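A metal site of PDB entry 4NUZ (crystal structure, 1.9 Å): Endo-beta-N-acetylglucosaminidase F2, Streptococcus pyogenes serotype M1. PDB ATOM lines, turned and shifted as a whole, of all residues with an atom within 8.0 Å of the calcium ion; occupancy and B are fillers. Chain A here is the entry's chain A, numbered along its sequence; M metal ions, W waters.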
ATOM      1  N   ASN A 686      22.380 -22.146   8.778  1.00  0.00           N
ATOM      2  CA  ASN A 686      22.786 -21.773   7.404  1.00  0.00           C
ATOM      3  C   ASN A 686      21.831 -22.399   6.335  1.00  0.00           C
ATOM      4  O   ASN A 686      21.441 -21.776   5.327  1.00  0.00           O
ATOM      5  CB  ASN A 686      24.266 -22.159   7.118  1.00  0.00           C
ATOM      6  CG  ASN A 686      25.301 -21.207   7.779  1.00  0.00           C
ATOM      7  OD1 ASN A 686      25.009 -20.044   8.118  1.00  0.00           O
ATOM      8  ND2 ASN A 686      26.527 -21.713   7.923  1.00  0.00           N
ATOM      9  N   ALA A 687      21.457 -23.636   6.592  1.00  0.00           N
ATOM     10  CA  ALA A 687      20.511 -24.342   5.747  1.00  0.00           C
ATOM     11  C   ALA A 687      19.329 -23.407   5.368  1.00  0.00           C
ATOM     12  O   ALA A 687      18.939 -23.314   4.211  1.00  0.00           O
ATOM     13  CB  ALA A 687      20.043 -25.614   6.425  1.00  0.00           C
ATOM     14  N   ARG A 688      18.818 -22.676   6.341  1.00  0.00           N
ATOM     15  CA  ARG A 688      17.605 -21.881   6.161  1.00  0.00           C
ATOM     16  C   ARG A 688      17.838 -20.720   5.177  1.00  0.00           C
ATOM     17  O   ARG A 688      16.876 -20.234   4.549  1.00  0.00           O
ATOM     18  CB  ARG A 688      17.108 -21.330   7.514  1.00  0.00           C
ATOM     19  CG  ARG A 688      17.649 -19.919   7.844  1.00  0.00           C
ATOM     20  CD  ARG A 688      17.037 -19.314   9.114  1.00  0.00           C
ATOM     21  NE  ARG A 688      17.045 -20.283  10.183  1.00  0.00           N
ATOM     22  CZ  ARG A 688      17.352 -20.023  11.452  1.00  0.00           C
ATOM     23  NH1 ARG A 688      17.689 -18.794  11.860  1.00  0.00           N
ATOM     24  NH2 ARG A 688      17.329 -21.022  12.308  1.00  0.00           N
ATOM     25  N   LYS A 689      19.093 -20.277   5.047  1.00  0.00           N
ATOM     26  CA  LYS A 689      19.438 -19.190   4.125  1.00  0.00           C
ATOM     27  C   LYS A 689      19.343 -19.649   2.674  1.00  0.00           C
ATOM     28  O   LYS A 689      19.393 -18.791   1.754  1.00  0.00           O
ATOM     29  CB  LYS A 689      20.856 -18.683   4.375  1.00  0.00           C
ATOM     30  CG  LYS A 689      21.062 -18.058   5.766  1.00  0.00           C
ATOM     31  CD  LYS A 689      22.564 -17.924   6.088  1.00  0.00           C
ATOM     32  CE  LYS A 689      22.788 -17.240   7.447  1.00  0.00           C
ATOM     33  NZ  LYS A 689      24.164 -16.671   7.620  1.00  0.00           N
ATOM     34  N   VAL A 690      19.294 -20.948   2.434  1.00  0.00           N
ATOM     35  CA  VAL A 690      18.996 -21.419   1.052  1.00  0.00           C
ATOM     36  C   VAL A 690      17.521 -21.174   0.711  1.00  0.00           C
ATOM     37  O   VAL A 690      17.096 -21.240  -0.475  1.00  0.00           O
ATOM     38  CB  VAL A 690      19.306 -22.912   0.788  1.00  0.00           C
ATOM     39  CG1 VAL A 690      20.595 -23.320   1.439  1.00  0.00           C
ATOM     40  CG2 VAL A 690      18.170 -23.750   1.234  1.00  0.00           C
ATOM     41  N   PHE A 691      16.755 -20.864   1.751  1.00  0.00           N
ATOM     42  CA  PHE A 691      15.350 -20.571   1.590  1.00  0.00           C
ATOM     43  C   PHE A 691      14.969 -19.096   1.791  1.00  0.00           C
ATOM     44  O   PHE A 691      13.763 -18.760   1.897  1.00  0.00           O
ATOM     45  CB  PHE A 691      14.564 -21.481   2.514  1.00  0.00           C
ATOM     46  CG  PHE A 691      14.818 -22.962   2.271  1.00  0.00           C
ATOM     47  CD1 PHE A 691      14.550 -23.534   1.031  1.00  0.00           C
ATOM     48  CD2 PHE A 691      15.299 -23.789   3.292  1.00  0.00           C
ATOM     49  CE1 PHE A 691      14.746 -24.923   0.822  1.00  0.00           C
ATOM     50  CE2 PHE A 691      15.525 -25.129   3.091  1.00  0.00           C
ATOM     51  CZ  PHE A 691      15.234 -25.720   1.853  1.00  0.00           C
ATOM     52  N   ASP A 692      15.944 -18.202   1.806  1.00  0.00           N
ATOM     53  CA  ASP A 692      15.648 -16.869   2.289  1.00  0.00           C
ATOM     54  C   ASP A 692      15.366 -15.859   1.180  1.00  0.00           C
ATOM     55  O   ASP A 692      15.278 -14.635   1.428  1.00  0.00           O
ATOM     56  CB  ASP A 692      16.757 -16.369   3.210  1.00  0.00           C
ATOM     57  CG  ASP A 692      18.057 -16.108   2.464  1.00  0.00           C
ATOM     58  OD1 ASP A 692      18.091 -16.282   1.221  1.00  0.00           O
ATOM     59  OD2 ASP A 692      19.041 -15.694   3.132  1.00  0.00           O
ATOM     60  N   GLY A 693      15.267 -16.367  -0.051  1.00  0.00           N
ATOM     61  CA  GLY A 693      14.858 -15.573  -1.206  1.00  0.00           C
ATOM     62  C   GLY A 693      15.872 -14.541  -1.659  1.00  0.00           C
ATOM     63  O   GLY A 693      15.497 -13.557  -2.323  1.00  0.00           O
ATOM     64  N   GLN A 694      17.146 -14.738  -1.329  1.00  0.00           N
ATOM     65  CA  GLN A 694      18.219 -13.829  -1.771  1.00  0.00           C
ATOM     66  C   GLN A 694      19.491 -14.637  -2.051  1.00  0.00           C
ATOM     67  O   GLN A 694      19.656 -15.743  -1.546  1.00  0.00           O
ATOM     68  CB  GLN A 694      18.509 -12.757  -0.707  1.00  0.00           C
ATOM     69  CG  GLN A 694      18.769 -13.346   0.698  1.00  0.00           C
ATOM     70  CD  GLN A 694      19.485 -12.400   1.668  1.00  0.00           C
ATOM     71  OE1 GLN A 694      19.120 -11.226   1.818  1.00  0.00           O
ATOM     72  NE2 GLN A 694      20.511 -12.918   2.351  1.00  0.00           N
ATOM     73  N   LEU A 695      20.418 -14.103  -2.844  1.00  0.00           N
ATOM     74  CA  LEU A 695      21.656 -14.840  -3.069  1.00  0.00           C
ATOM     75  C   LEU A 695      22.541 -14.771  -1.822  1.00  0.00           C
ATOM     76  O   LEU A 695      23.236 -15.738  -1.488  1.00  0.00           O
ATOM     77  CB  LEU A 695      22.381 -14.288  -4.299  1.00  0.00           C
ATOM     78  CG  LEU A 695      21.741 -14.746  -5.613  1.00  0.00           C
ATOM     79  CD1 LEU A 695      22.134 -13.832  -6.784  1.00  0.00           C
ATOM     80  CD2 LEU A 695      22.147 -16.193  -5.895  1.00  0.00           C
ATOM     81  N   GLY A 696      22.470 -13.647  -1.114  1.00  0.00           N
ATOM     82  CA  GLY A 696      23.313 -13.387   0.045  1.00  0.00           C
ATOM     83  C   GLY A 696      24.519 -12.522  -0.302  1.00  0.00           C
ATOM     84  O   GLY A 696      24.834 -12.335  -1.478  1.00  0.00           O
ATOM     85  N   SER A 697      25.203 -11.976   0.701  1.00  0.00           N
ATOM     86  CA  SER A 697      26.506 -11.334   0.479  1.00  0.00           C
ATOM     87  C   SER A 697      27.623 -12.347   0.709  1.00  0.00           C
ATOM     88  O   SER A 697      27.438 -13.320   1.439  1.00  0.00           O
ATOM     89  CB  SER A 697      26.699 -10.160   1.405  1.00  0.00           C
ATOM     90  OG  SER A 697      25.649  -9.230   1.239  1.00  0.00           O
ATOM     91  N   ASP A 700      28.629 -12.890   4.268  1.00  0.00           N
ATOM     92  CA  ASP A 700      27.919 -13.913   5.032  1.00  0.00           C
ATOM     93  C   ASP A 700      28.423 -15.313   4.717  1.00  0.00           C
ATOM     94  O   ASP A 700      28.484 -15.708   3.558  1.00  0.00           O
ATOM     95  CB  ASP A 700      26.415 -13.837   4.772  1.00  0.00           C
ATOM     96  CG  ASP A 700      25.595 -14.616   5.810  1.00  0.00           C
ATOM     97  OD1 ASP A 700      25.898 -14.495   7.021  1.00  0.00           O
ATOM     98  OD2 ASP A 700      24.659 -15.341   5.408  1.00  0.00           O
ATOM     99  N   ILE A 702      27.629 -18.857   4.188  1.00  0.00           N
ATOM    100  CA  ILE A 702      26.467 -19.684   3.901  1.00  0.00           C
ATOM    101  C   ILE A 702      26.860 -21.160   3.740  1.00  0.00           C
ATOM    102  O   ILE A 702      26.117 -21.924   3.135  1.00  0.00           O
ATOM    103  CB  ILE A 702      25.647 -19.195   2.652  1.00  0.00           C
ATOM    104  CG1 ILE A 702      26.370 -19.514   1.336  1.00  0.00           C
ATOM    105  CG2 ILE A 702      25.292 -17.700   2.757  1.00  0.00           C
ATOM    106  CD1 ILE A 702      25.591 -19.116   0.084  1.00  0.00           C
ATOM    107  N   PHE A 728      21.324 -23.108  -6.854  1.00  0.00           N
ATOM    108  CA  PHE A 728      22.403 -22.259  -7.302  1.00  0.00           C
ATOM    109  C   PHE A 728      23.774 -22.720  -6.745  1.00  0.00           C
ATOM    110  O   PHE A 728      23.901 -23.153  -5.583  1.00  0.00           O
ATOM    111  CB  PHE A 728      22.155 -20.778  -6.947  1.00  0.00           C
ATOM    112  CG  PHE A 728      20.949 -20.163  -7.629  1.00  0.00           C
ATOM    113  CD1 PHE A 728      19.654 -20.384  -7.138  1.00  0.00           C
ATOM    114  CD2 PHE A 728      21.117 -19.350  -8.744  1.00  0.00           C
ATOM    115  CE1 PHE A 728      18.545 -19.813  -7.750  1.00  0.00           C
ATOM    116  CE2 PHE A 728      20.015 -18.770  -9.383  1.00  0.00           C
ATOM    117  CZ  PHE A 728      18.725 -19.001  -8.883  1.00  0.00           C
ATOM    118  N   ARG A 733      26.613 -16.312  -6.678  1.00  0.00           N
ATOM    119  CA  ARG A 733      26.747 -15.224  -5.709  1.00  0.00           C
ATOM    120  C   ARG A 733      28.007 -14.402  -6.018  1.00  0.00           C
ATOM    121  O   ARG A 733      27.932 -13.198  -6.250  1.00  0.00           O
ATOM    122  CB  ARG A 733      26.772 -15.784  -4.273  1.00  0.00           C
ATOM    123  CG  ARG A 733      26.948 -14.708  -3.166  1.00  0.00           C
ATOM    124  CD  ARG A 733      27.136 -15.304  -1.766  1.00  0.00           C
ATOM    125  NE  ARG A 733      28.078 -16.440  -1.715  1.00  0.00           N
ATOM    126  CZ  ARG A 733      28.655 -16.880  -0.591  1.00  0.00           C
ATOM    127  NH1 ARG A 733      28.414 -16.289   0.583  1.00  0.00           N
ATOM    128  NH2 ARG A 733      29.507 -17.913  -0.624  1.00  0.00           N
ATOM    129  N   VAL A 817      25.633 -23.202  -1.207  1.00  0.00           N
ATOM    130  CA  VAL A 817      24.487 -22.970  -2.081  1.00  0.00           C
ATOM    131  C   VAL A 817      23.701 -21.700  -1.746  1.00  0.00           C
ATOM    132  O   VAL A 817      22.939 -21.660  -0.782  1.00  0.00           O
ATOM    133  CB  VAL A 817      23.524 -24.175  -1.971  1.00  0.00           C
ATOM    134  CG1 VAL A 817      22.303 -23.990  -2.895  1.00  0.00           C
ATOM    135  CG2 VAL A 817      24.266 -25.484  -2.259  1.00  0.00           C
ATOM    136  N   PRO A 818      23.853 -20.666  -2.560  1.00  0.00           N
ATOM    137  CA  PRO A 818      23.075 -19.435  -2.311  1.00  0.00           C
ATOM    138  C   PRO A 818      21.559 -19.628  -2.108  1.00  0.00           C
ATOM    139  O   PRO A 818      21.004 -18.946  -1.249  1.00  0.00           O
ATOM    140  CB  PRO A 818      23.340 -18.576  -3.561  1.00  0.00           C
ATOM    141  CG  PRO A 818      24.727 -19.039  -4.026  1.00  0.00           C
ATOM    142  CD  PRO A 818      24.835 -20.514  -3.656  1.00  0.00           C
ATOM    143  N   GLU A 819      20.916 -20.556  -2.831  1.00  0.00           N
ATOM    144  CA  GLU A 819      19.448 -20.671  -2.792  1.00  0.00           C
ATOM    145  C   GLU A 819      19.049 -21.978  -3.466  1.00  0.00           C
ATOM    146  O   GLU A 819      19.765 -22.446  -4.400  1.00  0.00           O
ATOM    147  CB  GLU A 819      18.787 -19.476  -3.508  1.00  0.00           C
ATOM    148  CG  GLU A 819      17.254 -19.408  -3.394  1.00  0.00           C
ATOM    149  CD  GLU A 819      16.748 -18.697  -2.125  1.00  0.00           C
ATOM    150  OE1 GLU A 819      15.511 -18.591  -1.960  1.00  0.00           O
ATOM    151  OE2 GLU A 819      17.598 -18.238  -1.311  1.00  0.00           O
ATOM    152  N   LEU A 820      17.951 -22.566  -2.968  1.00  0.00           N
ATOM    153  CA  LEU A 820      17.312 -23.774  -3.503  1.00  0.00           C
ATOM    154  C   LEU A 820      15.850 -23.429  -3.688  1.00  0.00           C
ATOM    155  O   LEU A 820      15.158 -23.072  -2.723  1.00  0.00           O
ATOM    156  CB  LEU A 820      17.445 -24.948  -2.544  1.00  0.00           C
ATOM    157  CG  LEU A 820      16.546 -26.196  -2.805  1.00  0.00           C
ATOM    158  CD1 LEU A 820      16.753 -26.786  -4.200  1.00  0.00           C
ATOM    159  CD2 LEU A 820      16.762 -27.353  -1.742  1.00  0.00           C
HETATM  160 CA    CA M   1      19.639 -17.472  -0.167  1.00  0.00          CA
HETATM  161  O   HOH W   1      21.825 -16.963   0.705  1.00  0.00           O
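The backbone carbonyl oxygen (O) of Glu 819 is in hydrogen-bond range of the backbone NH (N) of Phe 728, 3.0 Å away. The side-chain amino group (NZ) of Lys 689 is in salt-bridge range of the side-chain carboxylate (OD2) of Asp 700, at 2.6 Å. The side-chain carboxylate of Glu 819 is in hydrogen-bond range of the backbone NH of Gly 693, at 2.9 Å.
Five residues have an atom within 4 Å of the calcium ion: Lys 689, Asp 692, Gln 694, Pro 818 and Glu 819. The nearest printed residue that does not touch the calcium ion is Val 690 (4.2 Å).
The calcium ion is bound by the backbone carbonyl oxygen of Gln 694, the backbone carbonyl oxygen of Pro 818, the backbone carbonyl oxygen of Lys 689, the side-chain carboxylate of Asp 692, water W1 and the side-chain carboxylate of Glu 819.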
